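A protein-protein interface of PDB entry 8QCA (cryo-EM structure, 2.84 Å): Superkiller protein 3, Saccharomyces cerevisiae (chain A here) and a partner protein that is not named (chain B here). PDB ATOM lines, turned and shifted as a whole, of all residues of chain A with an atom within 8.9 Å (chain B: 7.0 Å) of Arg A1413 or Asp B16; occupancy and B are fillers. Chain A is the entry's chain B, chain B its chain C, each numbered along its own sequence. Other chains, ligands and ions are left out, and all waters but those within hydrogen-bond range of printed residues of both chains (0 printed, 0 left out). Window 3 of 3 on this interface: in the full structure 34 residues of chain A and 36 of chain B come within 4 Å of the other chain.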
ATOM      1  N   TYR A1406      16.468  17.687  25.163  1.00  0.00           N
ATOM      2  CA  TYR A1406      17.181  16.798  24.245  1.00  0.00           C
ATOM      3  C   TYR A1406      16.246  16.151  23.232  1.00  0.00           C
ATOM      4  O   TYR A1406      16.560  16.095  22.038  1.00  0.00           O
ATOM      5  CB  TYR A1406      17.943  15.723  25.023  1.00  0.00           C
ATOM      6  CG  TYR A1406      19.188  16.223  25.711  1.00  0.00           C
ATOM      7  CD1 TYR A1406      19.770  17.423  25.340  1.00  0.00           C
ATOM      8  CD2 TYR A1406      19.782  15.495  26.730  1.00  0.00           C
ATOM      9  CE1 TYR A1406      20.914  17.881  25.954  1.00  0.00           C
ATOM     10  CE2 TYR A1406      20.923  15.950  27.356  1.00  0.00           C
ATOM     11  CZ  TYR A1406      21.484  17.145  26.966  1.00  0.00           C
ATOM     12  OH  TYR A1406      22.621  17.604  27.586  1.00  0.00           O
ATOM     13  N   CYS A1407      15.097  15.651  23.683  1.00  0.00           N
ATOM     14  CA  CYS A1407      14.212  14.931  22.775  1.00  0.00           C
ATOM     15  C   CYS A1407      13.580  15.855  21.742  1.00  0.00           C
ATOM     16  O   CYS A1407      13.244  15.409  20.641  1.00  0.00           O
ATOM     17  CB  CYS A1407      13.130  14.200  23.565  1.00  0.00           C
ATOM     18  SG  CYS A1407      13.748  12.806  24.522  1.00  0.00           S
ATOM     19  N   SER A1409      14.800  18.042  19.866  1.00  0.00           N
ATOM     20  CA  SER A1409      15.580  18.252  18.655  1.00  0.00           C
ATOM     21  C   SER A1409      15.267  17.231  17.568  1.00  0.00           C
ATOM     22  O   SER A1409      15.759  17.380  16.446  1.00  0.00           O
ATOM     23  CB  SER A1409      17.074  18.221  18.980  1.00  0.00           C
ATOM     24  OG  SER A1409      17.503  16.905  19.269  1.00  0.00           O
ATOM     25  N   LYS A1410      14.469  16.205  17.879  1.00  0.00           N
ATOM     26  CA  LYS A1410      13.986  15.232  16.898  1.00  0.00           C
ATOM     27  C   LYS A1410      15.140  14.540  16.174  1.00  0.00           C
ATOM     28  O   LYS A1410      15.166  14.441  14.947  1.00  0.00           O
ATOM     29  CB  LYS A1410      13.033  15.894  15.900  1.00  0.00           C
ATOM     30  N   ASN A1411      16.102  14.052  16.953  1.00  0.00           N
ATOM     31  CA  ASN A1411      17.261  13.358  16.413  1.00  0.00           C
ATOM     32  C   ASN A1411      17.499  12.089  17.216  1.00  0.00           C
ATOM     33  O   ASN A1411      17.246  12.046  18.422  1.00  0.00           O
ATOM     34  CB  ASN A1411      18.508  14.252  16.441  1.00  0.00           C
ATOM     35  CG  ASN A1411      19.674  13.643  15.703  1.00  0.00           C
ATOM     36  OD1 ASN A1411      19.503  13.039  14.646  1.00  0.00           O
ATOM     37  ND2 ASN A1411      20.871  13.801  16.255  1.00  0.00           N
ATOM     38  N   LEU A1412      17.995  11.053  16.533  1.00  0.00           N
ATOM     39  CA  LEU A1412      18.155   9.748  17.171  1.00  0.00           C
ATOM     40  C   LEU A1412      19.144   9.810  18.329  1.00  0.00           C
ATOM     41  O   LEU A1412      18.891   9.262  19.407  1.00  0.00           O
ATOM     42  CB  LEU A1412      18.601   8.715  16.136  1.00  0.00           C
ATOM     43  CG  LEU A1412      18.653   7.260  16.607  1.00  0.00           C
ATOM     44  CD1 LEU A1412      17.318   6.834  17.191  1.00  0.00           C
ATOM     45  CD2 LEU A1412      19.057   6.341  15.467  1.00  0.00           C
ATOM     46  N   ARG A1413      20.280  10.478  18.124  1.00  0.00           N
ATOM     47  CA  ARG A1413      21.285  10.572  19.178  1.00  0.00           C
ATOM     48  C   ARG A1413      20.758  11.349  20.377  1.00  0.00           C
ATOM     49  O   ARG A1413      20.914  10.917  21.528  1.00  0.00           O
ATOM     50  CB  ARG A1413      22.549  11.225  18.624  1.00  0.00           C
ATOM     51  CG  ARG A1413      23.187  10.455  17.482  1.00  0.00           C
ATOM     52  CD  ARG A1413      24.293  11.254  16.820  1.00  0.00           C
ATOM     53  NE  ARG A1413      24.878  10.539  15.693  1.00  0.00           N
ATOM     54  CZ  ARG A1413      25.740  11.067  14.836  1.00  0.00           C
ATOM     55  NH1 ARG A1413      26.132  12.325  14.939  1.00  0.00           N
ATOM     56  NH2 ARG A1413      26.219  10.314  13.851  1.00  0.00           N
ATOM     57  N   SER A1414      20.108  12.486  20.126  1.00  0.00           N
ATOM     58  CA  SER A1414      19.574  13.290  21.218  1.00  0.00           C
ATOM     59  C   SER A1414      18.409  12.590  21.904  1.00  0.00           C
ATOM     60  O   SER A1414      18.238  12.712  23.121  1.00  0.00           O
ATOM     61  CB  SER A1414      19.146  14.658  20.696  1.00  0.00           C
ATOM     62  OG  SER A1414      20.255  15.374  20.182  1.00  0.00           O
ATOM     63  N   ILE A1415      17.595  11.857  21.144  1.00  0.00           N
ATOM     64  CA  ILE A1415      16.490  11.119  21.747  1.00  0.00           C
ATOM     65  C   ILE A1415      17.018  10.011  22.649  1.00  0.00           C
ATOM     66  O   ILE A1415      16.506   9.793  23.753  1.00  0.00           O
ATOM     67  CB  ILE A1415      15.553  10.576  20.653  1.00  0.00           C
ATOM     68  CG1 ILE A1415      14.537  11.646  20.255  1.00  0.00           C
ATOM     69  CG2 ILE A1415      14.841   9.327  21.123  1.00  0.00           C
ATOM     70  CD1 ILE A1415      13.768  11.322  19.002  1.00  0.00           C
ATOM     71  N   GLN A1416      18.057   9.300  22.202  1.00  0.00           N
ATOM     72  CA  GLN A1416      18.677   8.290  23.052  1.00  0.00           C
ATOM     73  C   GLN A1416      19.269   8.918  24.307  1.00  0.00           C
ATOM     74  O   GLN A1416      19.160   8.358  25.403  1.00  0.00           O
ATOM     75  CB  GLN A1416      19.750   7.533  22.269  1.00  0.00           C
ATOM     76  CG  GLN A1416      19.199   6.537  21.262  1.00  0.00           C
ATOM     77  CD  GLN A1416      20.287   5.882  20.436  1.00  0.00           C
ATOM     78  OE1 GLN A1416      21.363   6.445  20.251  1.00  0.00           O
ATOM     79  NE2 GLN A1416      20.010   4.685  19.938  1.00  0.00           N
ATOM     80  N   ARG A1417      19.889  10.091  24.166  1.00  0.00           N
ATOM     81  CA  ARG A1417      20.452  10.790  25.319  1.00  0.00           C
ATOM     82  C   ARG A1417      19.364  11.169  26.323  1.00  0.00           C
ATOM     83  O   ARG A1417      19.504  10.941  27.534  1.00  0.00           O
ATOM     84  CB  ARG A1417      21.199  12.029  24.832  1.00  0.00           C
ATOM     85  CG  ARG A1417      22.115  12.682  25.836  1.00  0.00           C
ATOM     86  CD  ARG A1417      22.802  13.861  25.183  1.00  0.00           C
ATOM     87  NE  ARG A1417      23.556  13.441  24.008  1.00  0.00           N
ATOM     88  CZ  ARG A1417      24.025  14.265  23.082  1.00  0.00           C
ATOM     89  NH1 ARG A1417      23.841  15.571  23.162  1.00  0.00           N
ATOM     90  NH2 ARG A1417      24.690  13.764  22.045  1.00  0.00           N
ATOM     91  N   GLY A1418      18.262  11.737  25.830  1.00  0.00           N
ATOM     92  CA  GLY A1418      17.190  12.160  26.711  1.00  0.00           C
ATOM     93  C   GLY A1418      16.429  11.009  27.332  1.00  0.00           C
ATOM     94  O   GLY A1418      15.870  11.150  28.424  1.00  0.00           O
ATOM     95  N   MET A1419      16.386   9.859  26.656  1.00  0.00           N
ATOM     96  CA  MET A1419      15.785   8.680  27.266  1.00  0.00           C
ATOM     97  C   MET A1419      16.720   8.037  28.282  1.00  0.00           C
ATOM     98  O   MET A1419      16.253   7.440  29.255  1.00  0.00           O
ATOM     99  CB  MET A1419      15.386   7.665  26.194  1.00  0.00           C
ATOM    100  CG  MET A1419      14.634   6.465  26.746  1.00  0.00           C
ATOM    101  SD  MET A1419      14.187   5.243  25.505  1.00  0.00           S
ATOM    102  CE  MET A1419      14.280   3.739  26.469  1.00  0.00           C
ATOM    103  N   PHE A1420      18.032   8.147  28.074  1.00  0.00           N
ATOM    104  CA  PHE A1420      18.973   7.676  29.082  1.00  0.00           C
ATOM    105  C   PHE A1420      18.906   8.532  30.338  1.00  0.00           C
ATOM    106  O   PHE A1420      19.043   8.016  31.454  1.00  0.00           O
ATOM    107  CB  PHE A1420      20.392   7.667  28.514  1.00  0.00           C
ATOM    108  CG  PHE A1420      21.397   7.001  29.409  1.00  0.00           C
ATOM    109  CD1 PHE A1420      21.426   5.625  29.536  1.00  0.00           C
ATOM    110  CD2 PHE A1420      22.314   7.753  30.120  1.00  0.00           C
ATOM    111  CE1 PHE A1420      22.349   5.012  30.357  1.00  0.00           C
ATOM    112  CE2 PHE A1420      23.240   7.145  30.941  1.00  0.00           C
ATOM    113  CZ  PHE A1420      23.256   5.774  31.059  1.00  0.00           C
ATOM    114  N   LEU A1432      11.337   7.758  20.718  1.00  0.00           N
ATOM    115  CA  LEU A1432      12.285   6.734  20.290  1.00  0.00           C
ATOM    116  C   LEU A1432      11.576   5.603  19.553  1.00  0.00           C
ATOM    117  O   LEU A1432      12.104   5.069  18.571  1.00  0.00           O
ATOM    118  CB  LEU A1432      13.071   6.204  21.490  1.00  0.00           C
ATOM    119  CG  LEU A1432      14.220   5.233  21.199  1.00  0.00           C
ATOM    120  CD1 LEU A1432      15.340   5.437  22.195  1.00  0.00           C
ATOM    121  CD2 LEU A1432      13.749   3.793  21.255  1.00  0.00           C
ATOM    122  N   CYS A1435      10.790   6.832  16.042  1.00  0.00           N
ATOM    123  CA  CYS A1435      11.897   6.971  15.099  1.00  0.00           C
ATOM    124  C   CYS A1435      11.871   5.850  14.066  1.00  0.00           C
ATOM    125  O   CYS A1435      11.548   6.073  12.895  1.00  0.00           O
ATOM    126  CB  CYS A1435      13.234   6.978  15.843  1.00  0.00           C
ATOM    127  SG  CYS A1435      13.535   8.421  16.880  1.00  0.00           S
ATOM    128  N   LYS B  13      36.599   9.733  18.738  1.00  0.00           N
ATOM    129  CA  LYS B  13      35.683   9.249  17.706  1.00  0.00           C
ATOM    130  C   LYS B  13      35.711   7.725  17.622  1.00  0.00           C
ATOM    131  O   LYS B  13      35.690   7.138  16.538  1.00  0.00           O
ATOM    132  CB  LYS B  13      35.999   9.880  16.348  1.00  0.00           C
ATOM    133  N   ALA B  14      35.768   7.080  18.790  1.00  0.00           N
ATOM    134  CA  ALA B  14      35.809   5.621  18.837  1.00  0.00           C
ATOM    135  C   ALA B  14      34.491   5.013  18.374  1.00  0.00           C
ATOM    136  O   ALA B  14      34.484   4.008  17.653  1.00  0.00           O
ATOM    137  CB  ALA B  14      36.152   5.154  20.250  1.00  0.00           C
ATOM    138  N   HIS B  15      33.372   5.601  18.780  1.00  0.00           N
ATOM    139  CA  HIS B  15      32.045   5.148  18.394  1.00  0.00           C
ATOM    140  C   HIS B  15      31.353   6.222  17.562  1.00  0.00           C
ATOM    141  O   HIS B  15      31.792   7.373  17.499  1.00  0.00           O
ATOM    142  CB  HIS B  15      31.206   4.808  19.631  1.00  0.00           C
ATOM    143  CG  HIS B  15      31.492   3.455  20.208  1.00  0.00           C
ATOM    144  ND1 HIS B  15      30.917   2.301  19.721  1.00  0.00           N
ATOM    145  CD2 HIS B  15      32.279   3.075  21.241  1.00  0.00           C
ATOM    146  CE1 HIS B  15      31.343   1.268  20.426  1.00  0.00           C
ATOM    147  NE2 HIS B  15      32.172   1.710  21.353  1.00  0.00           N
ATOM    148  N   ASP B  16      30.257   5.830  16.912  1.00  0.00           N
ATOM    149  CA  ASP B  16      29.481   6.755  16.096  1.00  0.00           C
ATOM    150  C   ASP B  16      28.398   7.484  16.877  1.00  0.00           C
ATOM    151  O   ASP B  16      27.851   8.471  16.374  1.00  0.00           O
ATOM    152  CB  ASP B  16      28.834   6.017  14.920  1.00  0.00           C
ATOM    153  CG  ASP B  16      29.766   5.882  13.734  1.00  0.00           C
ATOM    154  OD1 ASP B  16      30.583   6.800  13.512  1.00  0.00           O
ATOM    155  OD2 ASP B  16      29.682   4.860  13.023  1.00  0.00           O
ATOM    156  N   ALA B  17      28.075   7.028  18.083  1.00  0.00           N
ATOM    157  CA  ALA B  17      27.051   7.655  18.905  1.00  0.00           C
ATOM    158  C   ALA B  17      27.553   7.686  20.344  1.00  0.00           C
ATOM    159  O   ALA B  17      28.697   7.321  20.628  1.00  0.00           O
ATOM    160  CB  ALA B  17      25.712   6.920  18.766  1.00  0.00           C
ATOM    161  N   ASP B  18      26.687   8.127  21.255  1.00  0.00           N
ATOM    162  CA  ASP B  18      27.064   8.256  22.656  1.00  0.00           C
ATOM    163  C   ASP B  18      27.484   6.910  23.232  1.00  0.00           C
ATOM    164  O   ASP B  18      26.803   5.900  23.043  1.00  0.00           O
ATOM    165  CB  ASP B  18      25.898   8.824  23.463  1.00  0.00           C
ATOM    166  CG  ASP B  18      25.544  10.235  23.059  1.00  0.00           C
ATOM    167  OD1 ASP B  18      26.429  10.946  22.540  1.00  0.00           O
ATOM    168  OD2 ASP B  18      24.377  10.632  23.258  1.00  0.00           O
ATOM    169  N   ILE B  19      28.608   6.903  23.941  1.00  0.00           N
ATOM    170  CA  ILE B  19      29.080   5.717  24.642  1.00  0.00           C
ATOM    171  C   ILE B  19      28.523   5.786  26.059  1.00  0.00           C
ATOM    172  O   ILE B  19      28.977   6.591  26.875  1.00  0.00           O
ATOM    173  CB  ILE B  19      30.610   5.633  24.643  1.00  0.00           C
ATOM    174  CG1 ILE B  19      31.151   5.822  23.227  1.00  0.00           C
ATOM    175  CG2 ILE B  19      31.068   4.298  25.200  1.00  0.00           C
ATOM    176  CD1 ILE B  19      32.642   6.039  23.169  1.00  0.00           C
ATOM    177  N   PHE B  20      27.537   4.941  26.352  1.00  0.00           N
ATOM    178  CA  PHE B  20      26.778   5.055  27.591  1.00  0.00           C
ATOM    179  C   PHE B  20      27.367   4.259  28.744  1.00  0.00           C
ATOM    180  O   PHE B  20      27.107   4.597  29.903  1.00  0.00           O
ATOM    181  CB  PHE B  20      25.332   4.610  27.364  1.00  0.00           C
ATOM    182  CG  PHE B  20      24.525   5.574  26.552  1.00  0.00           C
ATOM    183  CD1 PHE B  20      24.211   6.823  27.049  1.00  0.00           C
ATOM    184  CD2 PHE B  20      24.084   5.231  25.288  1.00  0.00           C
ATOM    185  CE1 PHE B  20      23.468   7.713  26.303  1.00  0.00           C
ATOM    186  CE2 PHE B  20      23.341   6.117  24.537  1.00  0.00           C
ATOM    187  CZ  PHE B  20      23.032   7.359  25.045  1.00  0.00           C
ATOM    188  N   SER B  33      27.600   1.478  22.749  1.00  0.00           N
ATOM    189  CA  SER B  33      27.196   2.788  22.269  1.00  0.00           C
ATOM    190  C   SER B  33      25.769   2.726  21.743  1.00  0.00           C
ATOM    191  O   SER B  33      25.170   1.655  21.624  1.00  0.00           O
ATOM    192  CB  SER B  33      28.145   3.297  21.177  1.00  0.00           C
ATOM    193  OG  SER B  33      27.845   4.632  20.815  1.00  0.00           O
ATOM    194  N   GLY B  34      25.226   3.900  21.428  1.00  0.00           N
ATOM    195  CA  GLY B  34      23.885   3.989  20.888  1.00  0.00           C
ATOM    196  C   GLY B  34      23.752   3.621  19.428  1.00  0.00           C
ATOM    197  O   GLY B  34      22.627   3.536  18.927  1.00  0.00           O
ATOM    198  N   ASP B  35      24.866   3.402  18.733  1.00  0.00           N
ATOM    199  CA  ASP B  35      24.823   2.964  17.344  1.00  0.00           C
ATOM    200  C   ASP B  35      24.673   1.454  17.206  1.00  0.00           C
ATOM    201  O   ASP B  35      24.606   0.955  16.078  1.00  0.00           O
ATOM    202  CB  ASP B  35      26.077   3.436  16.599  1.00  0.00           C
ATOM    203  CG  ASP B  35      27.360   2.912  17.212  1.00  0.00           C
ATOM    204  OD1 ASP B  35      27.302   2.279  18.284  1.00  0.00           O
ATOM    205  OD2 ASP B  35      28.433   3.136  16.616  1.00  0.00           O
ATOM    206  N   TYR B  37      26.786  -1.037  18.325  1.00  0.00           N
ATOM    207  CA  TYR B  37      28.010  -1.815  18.237  1.00  0.00           C
ATOM    208  C   TYR B  37      28.572  -2.105  19.619  1.00  0.00           C
ATOM    209  O   TYR B  37      28.223  -1.463  20.613  1.00  0.00           O
ATOM    210  CB  TYR B  37      29.066  -1.102  17.387  1.00  0.00           C
ATOM    211  CG  TYR B  37      28.970  -1.416  15.915  1.00  0.00           C
ATOM    212  CD1 TYR B  37      29.813  -2.350  15.333  1.00  0.00           C
ATOM    213  CD2 TYR B  37      28.034  -0.787  15.109  1.00  0.00           C
ATOM    214  CE1 TYR B  37      29.731  -2.647  13.992  1.00  0.00           C
ATOM    215  CE2 TYR B  37      27.944  -1.078  13.765  1.00  0.00           C
ATOM    216  CZ  TYR B  37      28.795  -2.008  13.212  1.00  0.00           C
ATOM    217  OH  TYR B  37      28.712  -2.302  11.871  1.00  0.00           O
ATOM    218  N   ASP B 346      29.452  19.186  18.133  1.00  0.00           N
ATOM    219  CA  ASP B 346      28.557  18.072  17.865  1.00  0.00           C
ATOM    220  C   ASP B 346      27.844  18.285  16.530  1.00  0.00           C
ATOM    221  O   ASP B 346      28.219  19.145  15.728  1.00  0.00           O
ATOM    222  CB  ASP B 346      27.572  17.897  19.020  1.00  0.00           C
ATOM    223  CG  ASP B 346      26.494  18.964  19.040  1.00  0.00           C
ATOM    224  OD1 ASP B 346      26.767  20.100  18.601  1.00  0.00           O
ATOM    225  OD2 ASP B 346      25.370  18.668  19.498  1.00  0.00           O
ATOM    226  N   GLU B 347      26.805  17.490  16.273  1.00  0.00           N
ATOM    227  CA  GLU B 347      26.053  17.591  15.028  1.00  0.00           C
ATOM    228  C   GLU B 347      25.176  18.836  14.958  1.00  0.00           C
ATOM    229  O   GLU B 347      24.667  19.147  13.877  1.00  0.00           O
ATOM    230  CB  GLU B 347      25.192  16.340  14.835  1.00  0.00           C
ATOM    231  CG  GLU B 347      24.201  16.087  15.958  1.00  0.00           C
ATOM    232  CD  GLU B 347      24.773  15.207  17.054  1.00  0.00           C
ATOM    233  OE1 GLU B 347      25.998  14.972  17.053  1.00  0.00           O
ATOM    234  OE2 GLU B 347      23.997  14.757  17.923  1.00  0.00           O
ATOM    235  N   HIS B 348      24.984  19.548  16.068  1.00  0.00           N
ATOM    236  CA  HIS B 348      24.231  20.795  16.077  1.00  0.00           C
ATOM    237  C   HIS B 348      25.119  22.010  16.309  1.00  0.00           C
ATOM    238  O   HIS B 348      24.604  23.104  16.559  1.00  0.00           O
ATOM    239  CB  HIS B 348      23.131  20.748  17.139  1.00  0.00           C
ATOM    240  CG  HIS B 348      22.257  19.536  17.054  1.00  0.00           C
ATOM    241  ND1 HIS B 348      22.342  18.494  17.951  1.00  0.00           N
ATOM    242  CD2 HIS B 348      21.279  19.202  16.180  1.00  0.00           C
ATOM    243  CE1 HIS B 348      21.456  17.568  17.632  1.00  0.00           C
ATOM    244  NE2 HIS B 348      20.797  17.974  16.562  1.00  0.00           N
ATOM    245  N   ARG B 386      32.406  11.300  22.474  1.00  0.00           N
ATOM    246  CA  ARG B 386      32.549   9.989  21.837  1.00  0.00           C
ATOM    247  C   ARG B 386      34.001   9.517  21.867  1.00  0.00           C
ATOM    248  O   ARG B 386      34.574   9.124  20.850  1.00  0.00           O
ATOM    249  CB  ARG B 386      32.005  10.004  20.407  1.00  0.00           C
ATOM    250  CG  ARG B 386      30.495  10.054  20.326  1.00  0.00           C
ATOM    251  CD  ARG B 386      30.033  10.903  19.160  1.00  0.00           C
ATOM    252  NE  ARG B 386      30.852  10.686  17.974  1.00  0.00           N
ATOM    253  CZ  ARG B 386      30.666  11.300  16.813  1.00  0.00           C
ATOM    254  NH1 ARG B 386      29.692  12.181  16.647  1.00  0.00           N
ATOM    255  NH2 ARG B 386      31.474  11.023  15.795  1.00  0.00           N
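Of the printed residues of chain B, Phe A1420 touches Phe B20 (3.7 Å).
Asp B16 touches just one residue of chain A: Arg A1413 (3.5 Å).
No residue of chain A comes within 4 Å of Ala B17.
Of the printed residues of chain A, His B348 touches Ser A1414.
Printed residues of chain A within 4 Å of Arg B386: Arg A1413 (3.95 Å).
The nearest printed residue of chain B that does not touch Arg A1417 is Phe B20 (4.3 Å).
Among the printed residues, pairs that only touch across the chains: Arg A1413 with Asp B16, Ser A1414 with His B348, Asn A1411 with Glu B347, Phe A1420 with Phe B20, Arg A1413 with Asp B18 and Arg A1413 with Arg B386.
The side-chain carboxylate (OE1) of Glu B347 is in salt-bridge range of the guanidinium group (NH1) of Arg A1413.
The side-chain amide nitrogen of Gln A1416 sits at hydrogen-bond distance from the backbone carbonyl oxygen of Gly B34.
The guanidinium group (NE) of Arg A1417 is in salt-bridge range of the side-chain carboxylate (OD2) of Asp B18.
The backbone carbonyl oxygen (O) of Arg B386 lies within hydrogen-bond range of the backbone NH (N) of Lys B13.
O of His B15 lies within hydrogen-bond range of NE of Arg B386 (3.5 Å).
N of Asp B16 is in hydrogen-bond range of OD2 of Asp B35 (3.3 Å).
OG of Ser B33 sits at hydrogen-bond distance from O of Asp B18 (2.8 Å).
N of Gly B34 is in hydrogen-bond range of O of Asp B18, at 3.0 Å.
The side-chain carboxylate (OD1) of Asp B346 lies within hydrogen-bond range of the backbone NH (N) of His B348, at 3.1 Å.
Of the 16 printed residues of chain B, 7 touch a printed residue of chain A.
Of the 16 printed residues of chain A, 6 touch a printed residue of chain B.
Hydrophobic or aromatic side chains of chain A that line the printed part of chain B: Phe A1420.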
